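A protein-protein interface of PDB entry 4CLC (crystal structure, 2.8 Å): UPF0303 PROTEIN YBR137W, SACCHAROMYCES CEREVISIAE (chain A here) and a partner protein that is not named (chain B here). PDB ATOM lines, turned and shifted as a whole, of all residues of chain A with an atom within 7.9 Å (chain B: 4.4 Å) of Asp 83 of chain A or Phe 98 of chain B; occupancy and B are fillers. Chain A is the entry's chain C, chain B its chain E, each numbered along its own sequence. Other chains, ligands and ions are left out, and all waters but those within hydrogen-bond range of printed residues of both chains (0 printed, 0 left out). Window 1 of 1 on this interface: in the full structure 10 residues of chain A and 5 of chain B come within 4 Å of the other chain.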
ATOM      1  N   ALA A  60     -14.935   5.893  -9.501  1.00  0.00           N
ATOM      2  CA  ALA A  60     -15.175   6.549  -8.223  1.00  0.00           C
ATOM      3  C   ALA A  60     -14.435   5.807  -7.119  1.00  0.00           C
ATOM      4  O   ALA A  60     -14.494   4.587  -7.046  1.00  0.00           O
ATOM      5  CB  ALA A  60     -16.658   6.619  -7.939  1.00  0.00           C
ATOM      6  N   GLY A  79     -16.433  10.326 -16.605  1.00  0.00           N
ATOM      7  CA  GLY A  79     -17.673   9.859 -17.195  1.00  0.00           C
ATOM      8  C   GLY A  79     -18.586   9.296 -16.099  1.00  0.00           C
ATOM      9  O   GLY A  79     -19.471   8.513 -16.390  1.00  0.00           O
ATOM     10  N   SER A  80     -18.326   9.613 -14.833  1.00  0.00           N
ATOM     11  CA  SER A  80     -19.055   8.974 -13.720  1.00  0.00           C
ATOM     12  C   SER A  80     -20.507   9.438 -13.536  1.00  0.00           C
ATOM     13  O   SER A  80     -20.990  10.344 -14.215  1.00  0.00           O
ATOM     14  CB  SER A  80     -18.315   9.211 -12.409  1.00  0.00           C
ATOM     15  OG  SER A  80     -18.181  10.607 -12.166  1.00  0.00           O
ATOM     16  N   ALA A  81     -21.204   8.799 -12.606  1.00  0.00           N
ATOM     17  CA  ALA A  81     -22.633   9.034 -12.431  1.00  0.00           C
ATOM     18  C   ALA A  81     -23.086   8.534 -11.067  1.00  0.00           C
ATOM     19  O   ALA A  81     -22.378   7.764 -10.430  1.00  0.00           O
ATOM     20  CB  ALA A  81     -23.448   8.364 -13.557  1.00  0.00           C
ATOM     21  N   LEU A  82     -24.270   8.970 -10.642  1.00  0.00           N
ATOM     22  CA  LEU A  82     -24.805   8.612  -9.345  1.00  0.00           C
ATOM     23  C   LEU A  82     -24.752   7.126  -9.091  1.00  0.00           C
ATOM     24  O   LEU A  82     -24.484   6.704  -7.961  1.00  0.00           O
ATOM     25  CB  LEU A  82     -26.243   9.103  -9.214  1.00  0.00           C
ATOM     26  CG  LEU A  82     -27.026   8.800  -7.926  1.00  0.00           C
ATOM     27  CD1 LEU A  82     -26.396   9.440  -6.688  1.00  0.00           C
ATOM     28  CD2 LEU A  82     -28.441   9.250  -8.121  1.00  0.00           C
ATOM     29  N   ASP A  83     -24.970   6.329 -10.138  1.00  0.00           N
ATOM     30  CA  ASP A  83     -24.960   4.863  -9.999  1.00  0.00           C
ATOM     31  C   ASP A  83     -23.668   4.322  -9.373  1.00  0.00           C
ATOM     32  O   ASP A  83     -23.702   3.312  -8.671  1.00  0.00           O
ATOM     33  CB  ASP A  83     -25.209   4.177 -11.346  1.00  0.00           C
ATOM     34  CG  ASP A  83     -25.349   2.662 -11.203  1.00  0.00           C
ATOM     35  OD1 ASP A  83     -26.314   2.216 -10.528  1.00  0.00           O
ATOM     36  OD2 ASP A  83     -24.495   1.919 -11.753  1.00  0.00           O
ATOM     37  N   ASN A  84     -22.554   5.008  -9.624  1.00  0.00           N
ATOM     38  CA  ASN A  84     -21.304   4.799  -8.892  1.00  0.00           C
ATOM     39  C   ASN A  84     -21.458   4.864  -7.378  1.00  0.00           C
ATOM     40  O   ASN A  84     -20.828   4.105  -6.650  1.00  0.00           O
ATOM     41  CB  ASN A  84     -20.253   5.839  -9.301  1.00  0.00           C
ATOM     42  CG  ASN A  84     -19.638   5.559 -10.652  1.00  0.00           C
ATOM     43  OD1 ASN A  84     -19.811   6.334 -11.594  1.00  0.00           O
ATOM     44  ND2 ASN A  84     -18.914   4.440 -10.762  1.00  0.00           N
ATOM     45  N   ASP A  85     -22.281   5.794  -6.901  1.00  0.00           N
ATOM     46  CA  ASP A  85     -22.390   5.978  -5.466  1.00  0.00           C
ATOM     47  C   ASP A  85     -23.163   4.816  -4.889  1.00  0.00           C
ATOM     48  O   ASP A  85     -22.951   4.417  -3.743  1.00  0.00           O
ATOM     49  CB  ASP A  85     -23.050   7.311  -5.071  1.00  0.00           C
ATOM     50  CG  ASP A  85     -22.454   8.543  -5.777  1.00  0.00           C
ATOM     51  OD1 ASP A  85     -21.605   8.460  -6.693  1.00  0.00           O
ATOM     52  OD2 ASP A  85     -22.753   9.651  -5.297  1.00  0.00           O
ATOM     53  N   PHE A  86     -24.072   4.280  -5.693  1.00  0.00           N
ATOM     54  CA  PHE A  86     -24.867   3.134  -5.292  1.00  0.00           C
ATOM     55  C   PHE A  86     -23.981   1.893  -5.210  1.00  0.00           C
ATOM     56  O   PHE A  86     -24.052   1.122  -4.244  1.00  0.00           O
ATOM     57  CB  PHE A  86     -26.018   2.923  -6.266  1.00  0.00           C
ATOM     58  CG  PHE A  86     -27.255   3.703  -5.933  1.00  0.00           C
ATOM     59  CD1 PHE A  86     -28.129   3.253  -4.966  1.00  0.00           C
ATOM     60  CD2 PHE A  86     -27.573   4.862  -6.610  1.00  0.00           C
ATOM     61  CE1 PHE A  86     -29.259   3.957  -4.652  1.00  0.00           C
ATOM     62  CE2 PHE A  86     -28.731   5.558  -6.288  1.00  0.00           C
ATOM     63  CZ  PHE A  86     -29.554   5.098  -5.307  1.00  0.00           C
ATOM     64  N   TRP A  87     -23.135   1.698  -6.219  1.00  0.00           N
ATOM     65  CA  TRP A  87     -22.222   0.576  -6.173  1.00  0.00           C
ATOM     66  C   TRP A  87     -21.313   0.704  -4.987  1.00  0.00           C
ATOM     67  O   TRP A  87     -21.074  -0.284  -4.287  1.00  0.00           O
ATOM     68  CB  TRP A  87     -21.411   0.463  -7.452  1.00  0.00           C
ATOM     69  CG  TRP A  87     -22.172  -0.185  -8.556  1.00  0.00           C
ATOM     70  CD1 TRP A  87     -22.796   0.440  -9.590  1.00  0.00           C
ATOM     71  CD2 TRP A  87     -22.430  -1.583  -8.716  1.00  0.00           C
ATOM     72  NE1 TRP A  87     -23.407  -0.480 -10.393  1.00  0.00           N
ATOM     73  CE2 TRP A  87     -23.196  -1.730  -9.883  1.00  0.00           C
ATOM     74  CE3 TRP A  87     -22.080  -2.721  -7.992  1.00  0.00           C
ATOM     75  CZ2 TRP A  87     -23.606  -2.973 -10.355  1.00  0.00           C
ATOM     76  CZ3 TRP A  87     -22.494  -3.967  -8.470  1.00  0.00           C
ATOM     77  CH2 TRP A  87     -23.250  -4.073  -9.637  1.00  0.00           C
ATOM     78  N   ILE A  88     -20.834   1.922  -4.737  1.00  0.00           N
ATOM     79  CA  ILE A  88     -19.914   2.140  -3.631  1.00  0.00           C
ATOM     80  C   ILE A  88     -20.553   1.770  -2.305  1.00  0.00           C
ATOM     81  O   ILE A  88     -19.936   1.068  -1.522  1.00  0.00           O
ATOM     82  CB  ILE A  88     -19.392   3.585  -3.579  1.00  0.00           C
ATOM     83  CG1 ILE A  88     -18.354   3.788  -4.686  1.00  0.00           C
ATOM     84  CG2 ILE A  88     -18.729   3.854  -2.245  1.00  0.00           C
ATOM     85  CD1 ILE A  88     -17.887   5.229  -4.906  1.00  0.00           C
ATOM     86  N   GLN A  89     -21.794   2.190  -2.067  1.00  0.00           N
ATOM     87  CA  GLN A  89     -22.455   1.873  -0.798  1.00  0.00           C
ATOM     88  C   GLN A  89     -22.693   0.396  -0.716  1.00  0.00           C
ATOM     89  O   GLN A  89     -22.443  -0.250   0.292  1.00  0.00           O
ATOM     90  CB  GLN A  89     -23.785   2.626  -0.643  1.00  0.00           C
ATOM     91  CG  GLN A  89     -23.598   4.114  -0.343  1.00  0.00           C
ATOM     92  CD  GLN A  89     -22.540   4.389   0.748  1.00  0.00           C
ATOM     93  OE1 GLN A  89     -22.756   4.087   1.927  1.00  0.00           O
ATOM     94  NE2 GLN A  89     -21.391   4.952   0.345  1.00  0.00           N
ATOM     95  N   ARG A  90     -23.165  -0.130  -1.830  1.00  0.00           N
ATOM     96  CA  ARG A  90     -23.587  -1.502  -1.899  1.00  0.00           C
ATOM     97  C   ARG A  90     -22.432  -2.459  -1.688  1.00  0.00           C
ATOM     98  O   ARG A  90     -22.553  -3.342  -0.855  1.00  0.00           O
ATOM     99  CB  ARG A  90     -24.282  -1.738  -3.220  1.00  0.00           C
ATOM    100  CG  ARG A  90     -25.709  -1.302  -3.209  1.00  0.00           C
ATOM    101  CD  ARG A  90     -26.372  -1.589  -4.523  1.00  0.00           C
ATOM    102  NE  ARG A  90     -26.325  -3.004  -4.877  1.00  0.00           N
ATOM    103  CZ  ARG A  90     -25.719  -3.441  -5.974  1.00  0.00           C
ATOM    104  NH1 ARG A  90     -25.126  -2.548  -6.765  1.00  0.00           N
ATOM    105  NH2 ARG A  90     -25.704  -4.734  -6.273  1.00  0.00           N
ATOM    106  N   SER A 149     -15.072   1.666  -7.959  1.00  0.00           N
ATOM    107  CA  SER A 149     -16.194   1.363  -8.831  1.00  0.00           C
ATOM    108  C   SER A 149     -16.055   1.923 -10.258  1.00  0.00           C
ATOM    109  O   SER A 149     -15.720   3.094 -10.463  1.00  0.00           O
ATOM    110  CB  SER A 149     -17.491   1.883  -8.203  1.00  0.00           C
ATOM    111  OG  SER A 149     -18.481   2.167  -9.189  1.00  0.00           O
ATOM    112  N   THR B  94     -33.725   6.758 -14.575  1.00  0.00           N
ATOM    113  CA  THR B  94     -32.627   5.956 -15.116  1.00  0.00           C
ATOM    114  C   THR B  94     -31.540   6.791 -15.785  1.00  0.00           C
ATOM    115  O   THR B  94     -30.367   6.690 -15.432  1.00  0.00           O
ATOM    116  CB  THR B  94     -33.154   4.942 -16.116  1.00  0.00           C
ATOM    117  OG1 THR B  94     -34.061   4.063 -15.439  1.00  0.00           O
ATOM    118  CG2 THR B  94     -32.003   4.126 -16.713  1.00  0.00           C
ATOM    119  N   ALA B  95     -31.951   7.628 -16.735  1.00  0.00           N
ATOM    120  CA  ALA B  95     -31.045   8.546 -17.410  1.00  0.00           C
ATOM    121  C   ALA B  95     -30.192   9.340 -16.437  1.00  0.00           C
ATOM    122  O   ALA B  95     -29.031   9.604 -16.716  1.00  0.00           O
ATOM    123  CB  ALA B  95     -31.820   9.504 -18.297  1.00  0.00           C
ATOM    124  N   LEU B  96     -30.751   9.744 -15.302  1.00  0.00           N
ATOM    125  CA  LEU B  96     -29.976  10.565 -14.382  1.00  0.00           C
ATOM    126  C   LEU B  96     -29.000   9.743 -13.524  1.00  0.00           C
ATOM    127  O   LEU B  96     -27.843  10.141 -13.354  1.00  0.00           O
ATOM    128  CB  LEU B  96     -30.910  11.385 -13.511  1.00  0.00           C
ATOM    129  CG  LEU B  96     -31.772  12.387 -14.281  1.00  0.00           C
ATOM    130  CD1 LEU B  96     -32.863  12.922 -13.367  1.00  0.00           C
ATOM    131  CD2 LEU B  96     -30.934  13.525 -14.835  1.00  0.00           C
ATOM    132  N   ARG B  97     -29.445   8.599 -13.007  1.00  0.00           N
ATOM    133  CA  ARG B  97     -28.576   7.737 -12.191  1.00  0.00           C
ATOM    134  C   ARG B  97     -27.420   7.139 -12.985  1.00  0.00           C
ATOM    135  O   ARG B  97     -26.344   6.907 -12.453  1.00  0.00           O
ATOM    136  CB  ARG B  97     -29.384   6.594 -11.558  1.00  0.00           C
ATOM    137  CG  ARG B  97     -28.559   5.634 -10.722  1.00  0.00           C
ATOM    138  CD  ARG B  97     -29.396   4.528 -10.150  1.00  0.00           C
ATOM    139  NE  ARG B  97     -28.594   3.429  -9.628  1.00  0.00           N
ATOM    140  CZ  ARG B  97     -29.008   2.633  -8.656  1.00  0.00           C
ATOM    141  NH1 ARG B  97     -30.208   2.827  -8.120  1.00  0.00           N
ATOM    142  NH2 ARG B  97     -28.234   1.657  -8.222  1.00  0.00           N
ATOM    143  N   PHE B  98     -27.656   6.879 -14.261  1.00  0.00           N
ATOM    144  CA  PHE B  98     -26.666   6.227 -15.101  1.00  0.00           C
ATOM    145  C   PHE B  98     -26.228   7.271 -16.102  1.00  0.00           C
ATOM    146  O   PHE B  98     -26.904   8.268 -16.326  1.00  0.00           O
ATOM    147  CB  PHE B  98     -27.222   4.979 -15.807  1.00  0.00           C
ATOM    148  CG  PHE B  98     -27.839   3.951 -14.881  1.00  0.00           C
ATOM    149  CD1 PHE B  98     -29.202   4.003 -14.555  1.00  0.00           C
ATOM    150  CD2 PHE B  98     -27.072   2.915 -14.363  1.00  0.00           C
ATOM    151  CE1 PHE B  98     -29.767   3.056 -13.712  1.00  0.00           C
ATOM    152  CE2 PHE B  98     -27.635   1.961 -13.519  1.00  0.00           C
ATOM    153  CZ  PHE B  98     -28.973   2.031 -13.190  1.00  0.00           C
ATOM    154  N   GLY B  99     -25.069   7.102 -16.684  1.00  0.00           N
ATOM    155  CA  GLY B  99     -24.599   8.195 -17.512  1.00  0.00           C
ATOM    156  C   GLY B  99     -25.364   8.477 -18.795  1.00  0.00           C
ATOM    157  O   GLY B  99     -25.030   9.412 -19.504  1.00  0.00           O
ATOM    158  N   HIS B 100     -26.360   7.665 -19.123  1.00  0.00           N
ATOM    159  CA  HIS B 100     -26.847   7.632 -20.503  1.00  0.00           C
ATOM    160  C   HIS B 100     -28.350   7.597 -20.637  1.00  0.00           C
ATOM    161  O   HIS B 100     -29.072   7.500 -19.659  1.00  0.00           O
ATOM    162  CB  HIS B 100     -26.293   6.414 -21.228  1.00  0.00           C
ATOM    163  CG  HIS B 100     -24.892   6.058 -20.846  1.00  0.00           C
ATOM    164  ND1 HIS B 100     -24.587   5.379 -19.686  1.00  0.00           N
ATOM    165  CD2 HIS B 100     -23.714   6.269 -21.481  1.00  0.00           C
ATOM    166  CE1 HIS B 100     -23.281   5.193 -19.617  1.00  0.00           C
ATOM    167  NE2 HIS B 100     -22.729   5.723 -20.696  1.00  0.00           N
ATOM    168  N   MET B 105     -29.398   2.507 -22.027  1.00  0.00           N
ATOM    169  CA  MET B 105     -29.328   1.607 -20.891  1.00  0.00           C
ATOM    170  C   MET B 105     -30.201   0.359 -21.091  1.00  0.00           C
ATOM    171  O   MET B 105     -29.847  -0.737 -20.634  1.00  0.00           O
ATOM    172  CB  MET B 105     -29.710   2.356 -19.620  1.00  0.00           C
ATOM    173  CG  MET B 105     -28.671   3.392 -19.194  1.00  0.00           C
ATOM    174  SD  MET B 105     -27.092   2.679 -18.781  1.00  0.00           S
ATOM    175  CE  MET B 105     -27.615   1.415 -17.659  1.00  0.00           C
ATOM    176  N   PHE B 118     -28.606  -4.437 -13.242  1.00  0.00           N
ATOM    177  CA  PHE B 118     -28.329  -3.169 -12.591  1.00  0.00           C
ATOM    178  C   PHE B 118     -28.726  -3.088 -11.112  1.00  0.00           C
ATOM    179  O   PHE B 118     -28.297  -2.176 -10.406  1.00  0.00           O
ATOM    180  CB  PHE B 118     -29.007  -2.071 -13.377  1.00  0.00           C
ATOM    181  CG  PHE B 118     -28.656  -2.090 -14.824  1.00  0.00           C
ATOM    182  CD1 PHE B 118     -27.351  -1.898 -15.227  1.00  0.00           C
ATOM    183  CD2 PHE B 118     -29.629  -2.296 -15.785  1.00  0.00           C
ATOM    184  CE1 PHE B 118     -27.013  -1.906 -16.572  1.00  0.00           C
ATOM    185  CE2 PHE B 118     -29.301  -2.297 -17.130  1.00  0.00           C
ATOM    186  CZ  PHE B 118     -27.982  -2.102 -17.522  1.00  0.00           C
ATOM    187  N   TYR B 125     -37.313   2.165 -11.768  1.00  0.00           N
ATOM    188  CA  TYR B 125     -36.549   2.603 -12.954  1.00  0.00           C
ATOM    189  C   TYR B 125     -36.975   1.932 -14.279  1.00  0.00           C
ATOM    190  O   TYR B 125     -37.068   0.707 -14.358  1.00  0.00           O
ATOM    191  CB  TYR B 125     -35.062   2.325 -12.771  1.00  0.00           C
ATOM    192  CG  TYR B 125     -34.393   2.958 -11.590  1.00  0.00           C
ATOM    193  CD1 TYR B 125     -34.591   2.461 -10.317  1.00  0.00           C
ATOM    194  CD2 TYR B 125     -33.503   4.016 -11.757  1.00  0.00           C
ATOM    195  CE1 TYR B 125     -33.963   3.016  -9.237  1.00  0.00           C
ATOM    196  CE2 TYR B 125     -32.859   4.584 -10.677  1.00  0.00           C
ATOM    197  CZ  TYR B 125     -33.091   4.073  -9.414  1.00  0.00           C
ATOM    198  OH  TYR B 125     -32.456   4.606  -8.317  1.00  0.00           O
ATOM    199  N   PHE B 127     -36.228   0.781 -18.184  1.00  0.00           N
ATOM    200  CA  PHE B 127     -35.319   0.744 -19.311  1.00  0.00           C
ATOM    201  C   PHE B 127     -36.093   0.590 -20.619  1.00  0.00           C
ATOM    202  O   PHE B 127     -36.279  -0.508 -21.125  1.00  0.00           O
ATOM    203  CB  PHE B 127     -34.320  -0.380 -19.110  1.00  0.00           C
ATOM    204  CG  PHE B 127     -33.555  -0.278 -17.813  1.00  0.00           C
ATOM    205  CD1 PHE B 127     -34.147  -0.626 -16.611  1.00  0.00           C
ATOM    206  CD2 PHE B 127     -32.239   0.156 -17.805  1.00  0.00           C
ATOM    207  CE1 PHE B 127     -33.455  -0.529 -15.432  1.00  0.00           C
ATOM    208  CE2 PHE B 127     -31.539   0.246 -16.630  1.00  0.00           C
ATOM    209  CZ  PHE B 127     -32.148  -0.097 -15.434  1.00  0.00           C
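N of Leu 82 of chain A sits at hydrogen-bond distance from O of Arg 97 of chain B. The side-chain carboxylate (OD1) of Asp 83 of chain A is in salt-bridge range of the guanidinium group (NE) of Arg 97 of chain B (2.7 Å).
The backbone NH (N) of Ala 81 of chain A sits at hydrogen-bond distance from the side-chain amide oxygen (OD1) of Asn 84 of chain A (3.0 Å). NE1 of Trp 87 of chain A is in hydrogen-bond range of OD2 of Asp 83 of chain A, 3.0 Å away. NH1 of Arg 97 of chain B is in hydrogen-bond range of OH of Tyr 125 of chain B (2.9 Å).
Of the 11 printed residues of chain B, 3 touch a printed residue of chain A. Hydrophobic or aromatic side chains of chain B within 4 Å of the printed part of chain A: Phe 98. Among the printed residues, Asp or Glu carboxylates within 4 Å of a Lys or Arg side-chain nitrogen of the other chain: Asp 83 of chain A with Arg 97 of chain B.
Asp 83 of chain A touches two residues of chain B. Phe 98 of chain B touches just these residues of chain A: Ala 81 (3.9 Å) and Asp 83 (3.3 Å). Printed residues of chain A within 4 Å of Gly 99 of chain B: Ala 81 (3.7 Å). Of the printed residues of chain B, Ala 81 of chain A touches Arg 97, Phe 98 and Gly 99. Of the printed residues of chain B, Phe 86 of chain A touches Arg 97. The nearest printed residue of chain B that does not touch Asp 83 of chain A is Phe 118 of chain B (4.8 Å).
Among the printed residues, pairs that only touch across the chains: Phe 86 of chain A with Arg 97 of chain B (3.2 Å), Asp 83 of chain A with Phe 98 of chain B (3.3 Å), Ala 81 of chain A with Arg 97 of chain B (3.4 Å), Ala 81 of chain A with Gly 99 of chain B (3.7 Å) and Ala 81 of chain A with Phe 98 of chain B (3.9 Å).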
